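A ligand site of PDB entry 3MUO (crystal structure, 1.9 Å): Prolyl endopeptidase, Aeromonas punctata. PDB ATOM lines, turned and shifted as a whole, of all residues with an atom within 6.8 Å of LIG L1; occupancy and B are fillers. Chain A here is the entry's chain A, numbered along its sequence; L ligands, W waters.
A carbon (C9) of LIG L1 is covalently linked to the side-chain hydroxyl (OG) of Ser 541 (1.3 Å). The side-chain hydroxyl of Tyr 461 lies within hydrogen-bond range of an oxygen (O4) of LIG L1 (2.6 Å). NH1 of Arg 627 lies within hydrogen-bond range of O3 of LIG L1. The indole nitrogen (NE1) of Trp 582 lies within hydrogen-bond range of an oxygen (O2) of LIG L1, at 3.0 Å. N of Asn 542 sits at hydrogen-bond distance from O4 of LIG L1 (3.1 Å).
The backbone NH (N) of Val 567 lies within hydrogen-bond range of the backbone carbonyl oxygen (O) of Ser 541 (3.5 Å). OG of Ser 541 sits at hydrogen-bond distance from NE2 of His 660 (3.0 Å). The backbone NH of Ser 541 lies close to the backbone carbonyl oxygen of Val 565 (3.3 Å). The backbone carbonyl oxygen (O) of Tyr 461 lies close to the side-chain amide oxygen (OD1) of Asn 542 (3.1 Å). The guanidinium group (NE) of Arg 627 lies within salt-bridge range of the side-chain carboxylate (OD2) of Asp 153, at 2.8 Å. The side-chain amide nitrogen (ND2) of Asn 542 sits at hydrogen-bond distance from the side-chain hydroxyl (OH) of Tyr 586 (2.7 Å). OD1 of Asn 542 is in hydrogen-bond range of N of Gly 463 (3.5 Å). O of Gly 581 lies within hydrogen-bond range of N of Thr 256.
Residues that only touch LIG L1: Phe 464 (3.3 Å), Val 567 (3.4 Å), Tyr 586 (3.5 Å), Val 628 (3.5 Å), Thr 256 (3.7 Å) and His 660 (3.7 Å). Hydrophobic or aromatic side chains within 4 Å of LIG L1: Tyr 461, Phe 464, Val 567, Trp 582 and Val 628. Of the 22 residues printed, 11 come within 4 Å of LIG L1. The nearest printed residue that does not touch LIG L1 is Tyr 236 (4.3 Å).
Water W3 lies within hydrogen-bond range of O2 of LIG L1 and OH of Tyr 236. Water W1 lies within hydrogen-bond range of O3 of LIG L1 (2.8 Å), NE2 of His 660 (2.8 Å) and OG of Ser 541 (3.3 Å). Water W2 bridges OH of Tyr 461 and O4 of LIG L1.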
ATOM      1  N   ASP A 153       6.525 -14.580  -6.610  1.00  0.00           N
ATOM      2  CA  ASP A 153       7.182 -14.136  -5.381  1.00  0.00           C
ATOM      3  C   ASP A 153       6.733 -14.976  -4.166  1.00  0.00           C
ATOM      4  O   ASP A 153       7.382 -14.942  -3.116  1.00  0.00           O
ATOM      5  CB  ASP A 153       6.859 -12.657  -5.082  1.00  0.00           C
ATOM      6  CG  ASP A 153       7.729 -11.678  -5.880  1.00  0.00           C
ATOM      7  OD1 ASP A 153       8.859 -12.028  -6.269  1.00  0.00           O
ATOM      8  OD2 ASP A 153       7.269 -10.527  -6.075  1.00  0.00           O
ATOM      9  N   PHE A 177       8.710 -12.634   0.409  1.00  0.00           N
ATOM     10  CA  PHE A 177       9.745 -11.645   0.760  1.00  0.00           C
ATOM     11  C   PHE A 177      10.281 -11.988   2.140  1.00  0.00           C
ATOM     12  O   PHE A 177      10.326 -11.140   3.043  1.00  0.00           O
ATOM     13  CB  PHE A 177       9.154 -10.212   0.807  1.00  0.00           C
ATOM     14  CG  PHE A 177       8.505  -9.775  -0.464  1.00  0.00           C
ATOM     15  CD1 PHE A 177       9.033 -10.108  -1.703  1.00  0.00           C
ATOM     16  CD2 PHE A 177       7.358  -8.969  -0.428  1.00  0.00           C
ATOM     17  CE1 PHE A 177       8.446  -9.657  -2.888  1.00  0.00           C
ATOM     18  CE2 PHE A 177       6.767  -8.513  -1.591  1.00  0.00           C
ATOM     19  CZ  PHE A 177       7.301  -8.863  -2.831  1.00  0.00           C
ATOM     20  N   TYR A 236       6.319  -4.416   4.504  1.00  0.00           N
ATOM     21  CA  TYR A 236       7.486  -5.299   4.447  1.00  0.00           C
ATOM     22  C   TYR A 236       8.112  -5.447   5.825  1.00  0.00           C
ATOM     23  O   TYR A 236       8.426  -4.438   6.479  1.00  0.00           O
ATOM     24  CB  TYR A 236       8.561  -4.719   3.510  1.00  0.00           C
ATOM     25  CG  TYR A 236       8.100  -4.357   2.113  1.00  0.00           C
ATOM     26  CD1 TYR A 236       7.787  -5.338   1.167  1.00  0.00           C
ATOM     27  CD2 TYR A 236       8.026  -3.012   1.712  1.00  0.00           C
ATOM     28  CE1 TYR A 236       7.425  -4.992  -0.169  1.00  0.00           C
ATOM     29  CE2 TYR A 236       7.667  -2.653   0.396  1.00  0.00           C
ATOM     30  CZ  TYR A 236       7.373  -3.646  -0.530  1.00  0.00           C
ATOM     31  OH  TYR A 236       7.046  -3.282  -1.814  1.00  0.00           O
ATOM     32  N   THR A 256      10.169   0.731  -0.695  1.00  0.00           N
ATOM     33  CA  THR A 256      11.474   0.153  -1.011  1.00  0.00           C
ATOM     34  C   THR A 256      12.649   1.017  -0.538  1.00  0.00           C
ATOM     35  O   THR A 256      13.798   0.621  -0.664  1.00  0.00           O
ATOM     36  CB  THR A 256      11.594  -0.140  -2.526  1.00  0.00           C
ATOM     37  OG1 THR A 256      11.171   1.009  -3.266  1.00  0.00           O
ATOM     38  CG2 THR A 256      10.708  -1.340  -2.909  1.00  0.00           C
ATOM     39  N   TYR A 461      17.717   1.242 -16.459  1.00  0.00           N
ATOM     40  CA  TYR A 461      16.731   0.892 -15.425  1.00  0.00           C
ATOM     41  C   TYR A 461      16.320   2.272 -14.913  1.00  0.00           C
ATOM     42  O   TYR A 461      15.267   2.802 -15.293  1.00  0.00           O
ATOM     43  CB  TYR A 461      17.394   0.040 -14.343  1.00  0.00           C
ATOM     44  CG  TYR A 461      16.434  -0.436 -13.273  1.00  0.00           C
ATOM     45  CD1 TYR A 461      15.532  -1.484 -13.516  1.00  0.00           C
ATOM     46  CD2 TYR A 461      16.453   0.138 -12.003  1.00  0.00           C
ATOM     47  CE1 TYR A 461      14.676  -1.942 -12.508  1.00  0.00           C
ATOM     48  CE2 TYR A 461      15.626  -0.316 -10.991  1.00  0.00           C
ATOM     49  CZ  TYR A 461      14.741  -1.352 -11.244  1.00  0.00           C
ATOM     50  OH  TYR A 461      13.958  -1.811 -10.201  1.00  0.00           O
ATOM     51  N   GLY A 463      16.172   3.884 -11.306  1.00  0.00           N
ATOM     52  CA  GLY A 463      15.254   4.062 -10.202  1.00  0.00           C
ATOM     53  C   GLY A 463      15.546   3.126  -9.048  1.00  0.00           C
ATOM     54  O   GLY A 463      16.394   2.232  -9.146  1.00  0.00           O
ATOM     55  N   PHE A 464      14.868   3.380  -7.938  1.00  0.00           N
ATOM     56  CA  PHE A 464      14.952   2.550  -6.741  1.00  0.00           C
ATOM     57  C   PHE A 464      16.313   2.372  -6.101  1.00  0.00           C
ATOM     58  O   PHE A 464      16.528   1.408  -5.364  1.00  0.00           O
ATOM     59  CB  PHE A 464      14.316   1.191  -7.056  1.00  0.00           C
ATOM     60  CG  PHE A 464      12.877   1.291  -7.464  1.00  0.00           C
ATOM     61  CD1 PHE A 464      11.859   1.339  -6.509  1.00  0.00           C
ATOM     62  CD2 PHE A 464      12.547   1.502  -8.807  1.00  0.00           C
ATOM     63  CE1 PHE A 464      10.542   1.603  -6.879  1.00  0.00           C
ATOM     64  CE2 PHE A 464      11.229   1.778  -9.184  1.00  0.00           C
ATOM     65  CZ  PHE A 464      10.230   1.826  -8.217  1.00  0.00           C
ATOM     66  N   VAL A 466      18.883   1.452  -7.399  1.00  0.00           N
ATOM     67  CA  VAL A 466      19.539   0.295  -7.988  1.00  0.00           C
ATOM     68  C   VAL A 466      20.702   0.784  -8.855  1.00  0.00           C
ATOM     69  O   VAL A 466      20.549   1.708  -9.648  1.00  0.00           O
ATOM     70  CB  VAL A 466      18.562  -0.522  -8.863  1.00  0.00           C
ATOM     71  CG1 VAL A 466      19.325  -1.560  -9.689  1.00  0.00           C
ATOM     72  CG2 VAL A 466      17.521  -1.195  -7.970  1.00  0.00           C
ATOM     73  N   GLY A 540      13.743  -3.647 -18.047  1.00  0.00           N
ATOM     74  CA  GLY A 540      12.754  -4.483 -17.396  1.00  0.00           C
ATOM     75  C   GLY A 540      12.254  -3.915 -16.089  1.00  0.00           C
ATOM     76  O   GLY A 540      13.019  -3.271 -15.369  1.00  0.00           O
ATOM     77  N   SER A 541      10.984  -4.178 -15.779  1.00  0.00           N
ATOM     78  CA  SER A 541      10.336  -3.684 -14.538  1.00  0.00           C
ATOM     79  C   SER A 541      10.346  -2.161 -14.577  1.00  0.00           C
ATOM     80  O   SER A 541       9.645  -1.563 -15.405  1.00  0.00           O
ATOM     81  CB  SER A 541      11.079  -4.229 -13.304  1.00  0.00           C
ATOM     82  OG  SER A 541      10.200  -4.312 -12.183  1.00  0.00           O
ATOM     83  N   ASN A 542      11.105  -1.509 -13.708  1.00  0.00           N
ATOM     84  CA  ASN A 542      11.169  -0.054 -13.780  1.00  0.00           C
ATOM     85  C   ASN A 542      11.822   0.326 -15.140  1.00  0.00           C
ATOM     86  O   ASN A 542      11.556   1.394 -15.718  1.00  0.00           O
ATOM     87  CB  ASN A 542      12.008   0.476 -12.602  1.00  0.00           C
ATOM     88  CG  ASN A 542      12.307   1.956 -12.709  1.00  0.00           C
ATOM     89  OD1 ASN A 542      13.467   2.358 -12.825  1.00  0.00           O
ATOM     90  ND2 ASN A 542      11.269   2.768 -12.685  1.00  0.00           N
ATOM     91  N   GLY A 543      12.651  -0.576 -15.656  1.00  0.00           N
ATOM     92  CA  GLY A 543      13.268  -0.374 -16.950  1.00  0.00           C
ATOM     93  C   GLY A 543      12.244  -0.589 -18.059  1.00  0.00           C
ATOM     94  O   GLY A 543      12.414  -0.107 -19.182  1.00  0.00           O
ATOM     95  N   VAL A 565       8.443  -7.027 -18.559  1.00  0.00           N
ATOM     96  CA  VAL A 565       7.704  -6.997 -17.294  1.00  0.00           C
ATOM     97  C   VAL A 565       7.614  -5.582 -16.727  1.00  0.00           C
ATOM     98  O   VAL A 565       7.874  -5.340 -15.546  1.00  0.00           O
ATOM     99  CB  VAL A 565       8.348  -7.964 -16.263  1.00  0.00           C
ATOM    100  CG1 VAL A 565       8.159  -9.402 -16.733  1.00  0.00           C
ATOM    101  CG2 VAL A 565       9.850  -7.652 -16.081  1.00  0.00           C
ATOM    102  N   GLY A 566       7.187  -4.652 -17.582  1.00  0.00           N
ATOM    103  CA  GLY A 566       7.136  -3.258 -17.176  1.00  0.00           C
ATOM    104  C   GLY A 566       5.931  -2.717 -16.442  1.00  0.00           C
ATOM    105  O   GLY A 566       4.820  -3.251 -16.534  1.00  0.00           O
ATOM    106  N   VAL A 567       6.176  -1.658 -15.690  1.00  0.00           N
ATOM    107  CA  VAL A 567       5.092  -0.972 -14.988  1.00  0.00           C
ATOM    108  C   VAL A 567       4.678   0.007 -16.088  1.00  0.00           C
ATOM    109  O   VAL A 567       5.461   0.874 -16.466  1.00  0.00           O
ATOM    110  CB  VAL A 567       5.615  -0.208 -13.753  1.00  0.00           C
ATOM    111  CG1 VAL A 567       4.450   0.407 -12.984  1.00  0.00           C
ATOM    112  CG2 VAL A 567       6.381  -1.169 -12.872  1.00  0.00           C
ATOM    113  N   ALA A 578       2.118  -5.812  -4.167  1.00  0.00           N
ATOM    114  CA  ALA A 578       2.805  -4.892  -3.247  1.00  0.00           C
ATOM    115  C   ALA A 578       3.269  -3.624  -3.972  1.00  0.00           C
ATOM    116  O   ALA A 578       4.189  -2.938  -3.520  1.00  0.00           O
ATOM    117  CB  ALA A 578       4.015  -5.603  -2.581  1.00  0.00           C
ATOM    118  N   GLY A 581       4.372  -0.275  -2.545  1.00  0.00           N
ATOM    119  CA  GLY A 581       5.710  -0.161  -1.982  1.00  0.00           C
ATOM    120  C   GLY A 581       6.633   0.684  -2.867  1.00  0.00           C
ATOM    121  O   GLY A 581       7.732   1.042  -2.441  1.00  0.00           O
ATOM    122  N   TRP A 582       6.207   0.990  -4.088  1.00  0.00           N
ATOM    123  CA  TRP A 582       7.021   1.811  -5.002  1.00  0.00           C
ATOM    124  C   TRP A 582       6.636   3.278  -4.988  1.00  0.00           C
ATOM    125  O   TRP A 582       7.174   4.065  -5.770  1.00  0.00           O
ATOM    126  CB  TRP A 582       6.908   1.298  -6.448  1.00  0.00           C
ATOM    127  CG  TRP A 582       7.067  -0.189  -6.557  1.00  0.00           C
ATOM    128  CD1 TRP A 582       7.848  -0.986  -5.776  1.00  0.00           C
ATOM    129  CD2 TRP A 582       6.371  -1.064  -7.456  1.00  0.00           C
ATOM    130  NE1 TRP A 582       7.668  -2.306  -6.122  1.00  0.00           N
ATOM    131  CE2 TRP A 582       6.771  -2.382  -7.149  1.00  0.00           C
ATOM    132  CE3 TRP A 582       5.442  -0.857  -8.495  1.00  0.00           C
ATOM    133  CZ2 TRP A 582       6.265  -3.505  -7.834  1.00  0.00           C
ATOM    134  CZ3 TRP A 582       4.937  -1.968  -9.174  1.00  0.00           C
ATOM    135  CH2 TRP A 582       5.359  -3.273  -8.834  1.00  0.00           C
ATOM    136  N   TYR A 586       7.825   6.544  -7.299  1.00  0.00           N
ATOM    137  CA  TYR A 586       6.875   7.029  -8.302  1.00  0.00           C
ATOM    138  C   TYR A 586       5.850   8.074  -7.888  1.00  0.00           C
ATOM    139  O   TYR A 586       5.454   8.898  -8.715  1.00  0.00           O
ATOM    140  CB  TYR A 586       6.068   5.852  -8.872  1.00  0.00           C
ATOM    141  CG  TYR A 586       6.869   4.764  -9.565  1.00  0.00           C
ATOM    142  CD1 TYR A 586       8.036   5.070 -10.270  1.00  0.00           C
ATOM    143  CD2 TYR A 586       6.398   3.441  -9.608  1.00  0.00           C
ATOM    144  CE1 TYR A 586       8.713   4.093 -11.002  1.00  0.00           C
ATOM    145  CE2 TYR A 586       7.068   2.455 -10.338  1.00  0.00           C
ATOM    146  CZ  TYR A 586       8.219   2.785 -11.042  1.00  0.00           C
ATOM    147  OH  TYR A 586       8.863   1.828 -11.806  1.00  0.00           O
ATOM    148  N   ARG A 627       5.075  -9.659  -9.125  1.00  0.00           N
ATOM    149  CA  ARG A 627       5.822  -8.476  -8.676  1.00  0.00           C
ATOM    150  C   ARG A 627       5.157  -7.299  -9.404  1.00  0.00           C
ATOM    151  O   ARG A 627       4.667  -6.356  -8.771  1.00  0.00           O
ATOM    152  CB  ARG A 627       7.299  -8.557  -9.063  1.00  0.00           C
ATOM    153  CG  ARG A 627       8.133  -7.326  -8.625  1.00  0.00           C
ATOM    154  CD  ARG A 627       8.342  -7.294  -7.105  1.00  0.00           C
ATOM    155  NE  ARG A 627       9.043  -8.493  -6.672  1.00  0.00           N
ATOM    156  CZ  ARG A 627      10.363  -8.642  -6.697  1.00  0.00           C
ATOM    157  NH1 ARG A 627      11.148  -7.658  -7.115  1.00  0.00           N
ATOM    158  NH2 ARG A 627      10.899  -9.805  -6.340  1.00  0.00           N
ATOM    159  N   VAL A 628       5.150  -7.369 -10.733  1.00  0.00           N
ATOM    160  CA  VAL A 628       4.524  -6.372 -11.609  1.00  0.00           C
ATOM    161  C   VAL A 628       3.472  -7.186 -12.376  1.00  0.00           C
ATOM    162  O   VAL A 628       3.821  -7.980 -13.254  1.00  0.00           O
ATOM    163  CB  VAL A 628       5.539  -5.756 -12.619  1.00  0.00           C
ATOM    164  CG1 VAL A 628       4.832  -4.769 -13.543  1.00  0.00           C
ATOM    165  CG2 VAL A 628       6.656  -5.055 -11.877  1.00  0.00           C
ATOM    166  N   HIS A 660       8.458 -12.839 -12.564  1.00  0.00           N
ATOM    167  CA  HIS A 660       9.177 -11.604 -12.825  1.00  0.00           C
ATOM    168  C   HIS A 660      10.550 -11.846 -13.452  1.00  0.00           C
ATOM    169  O   HIS A 660      11.016 -11.034 -14.255  1.00  0.00           O
ATOM    170  CB  HIS A 660       9.305 -10.786 -11.547  1.00  0.00           C
ATOM    171  CG  HIS A 660       9.606  -9.334 -11.781  1.00  0.00           C
ATOM    172  ND1 HIS A 660       8.822  -8.538 -12.591  1.00  0.00           N
ATOM    173  CD2 HIS A 660      10.600  -8.550 -11.312  1.00  0.00           C
ATOM    174  CE1 HIS A 660       9.320  -7.314 -12.606  1.00  0.00           C
ATOM    175  NE2 HIS A 660      10.401  -7.290 -11.840  1.00  0.00           N
HETATM  176  O1  LIG L   1      10.989  -5.340  -3.791  1.00  0.00           O
HETATM  177  C1  LIG L   1      10.666  -4.544  -4.831  1.00  0.00           C
HETATM  178  O2  LIG L   1       9.490  -4.452  -5.170  1.00  0.00           O
HETATM  179  N1  LIG L   1      11.642  -3.859  -5.483  1.00  0.00           N
HETATM  180  C2  LIG L   1      11.466  -2.945  -6.629  1.00  0.00           C
HETATM  181  C3  LIG L   1      10.874  -3.647  -7.865  1.00  0.00           C
HETATM  182  O3  LIG L   1      11.004  -4.858  -8.008  1.00  0.00           O
HETATM  183  C4  LIG L   1      12.873  -2.403  -6.998  1.00  0.00           C
HETATM  184  C5  LIG L   1      13.837  -3.453  -6.415  1.00  0.00           C
HETATM  185  C6  LIG L   1      13.086  -3.909  -5.141  1.00  0.00           C
HETATM  186  C7  LIG L   1       8.481  -2.399 -10.456  1.00  0.00           C
HETATM  187  C8  LIG L   1       9.152  -1.097  -9.980  1.00  0.00           C
HETATM  188  C9  LIG L   1      10.565  -3.600 -11.206  1.00  0.00           C
HETATM  189  O4  LIG L   1      11.763  -2.859 -11.030  1.00  0.00           O
HETATM  190  N2  LIG L   1      10.192  -2.925  -8.791  1.00  0.00           N
HETATM  191  C10 LIG L   1       9.952  -1.446  -8.729  1.00  0.00           C
HETATM  192  C11 LIG L   1       9.553  -3.448 -10.055  1.00  0.00           C
HETATM  193  C1  LG2 L   2      15.058  -6.132 -14.869  1.00  0.00           C
HETATM  194  C2  LG2 L   2      14.580  -6.209 -13.545  1.00  0.00           C
HETATM  195  C3  LG2 L   2      13.607  -7.164 -13.199  1.00  0.00           C
HETATM  196  C4  LG2 L   2      13.106  -8.051 -14.176  1.00  0.00           C
HETATM  197  C5  LG2 L   2      13.583  -7.987 -15.507  1.00  0.00           C
HETATM  198  C6  LG2 L   2      14.551  -7.027 -15.846  1.00  0.00           C
HETATM  199  C7  LG2 L   2      15.072  -6.953 -17.260  1.00  0.00           C
HETATM  200  O1  LG2 L   2      16.425  -7.463 -17.307  1.00  0.00           O
HETATM  201  C8  LG2 L   2      17.118  -7.498 -18.467  1.00  0.00           C
HETATM  202  O2  LG2 L   2      16.598  -7.079 -19.510  1.00  0.00           O
HETATM  203  N1  LG2 L   2      18.397  -8.002 -18.498  1.00  0.00           N
HETATM  204  C9  LG2 L   2      19.266  -8.093 -19.684  1.00  0.00           C
HETATM  205  C10 LG2 L   2      18.606  -8.904 -20.795  1.00  0.00           C
HETATM  206  O3  LG2 L   2      17.873  -9.827 -20.485  1.00  0.00           O
HETATM  207  C11 LG2 L   2      20.599  -8.730 -19.234  1.00  0.00           C
HETATM  208  C12 LG2 L   2      20.220  -9.486 -17.929  1.00  0.00           C
HETATM  209  C13 LG2 L   2      19.150  -8.538 -17.330  1.00  0.00           C
HETATM  210  C14 LG2 L   2      18.414  -8.484 -24.581  1.00  0.00           C
HETATM  211  C15 LG2 L   2      19.589  -7.564 -24.166  1.00  0.00           C
HETATM  212  C16 LG2 L   2      18.770 -10.733 -23.473  1.00  0.00           C
HETATM  213  O4  LG2 L   2      17.732 -11.707 -23.489  1.00  0.00           O
HETATM  214  N2  LG2 L   2      18.795  -8.608 -22.129  1.00  0.00           N
HETATM  215  C17 LG2 L   2      19.658  -7.506 -22.644  1.00  0.00           C
HETATM  216  C18 LG2 L   2      18.176  -9.345 -23.296  1.00  0.00           C
HETATM  217  O   HOH W   1      12.240  -6.040 -10.178  1.00  0.00           O
HETATM  218  O   HOH W   2      14.498  -4.445 -10.142  1.00  0.00           O
HETATM  219  O   HOH W   3       7.061  -5.116  -4.068  1.00  0.00           O
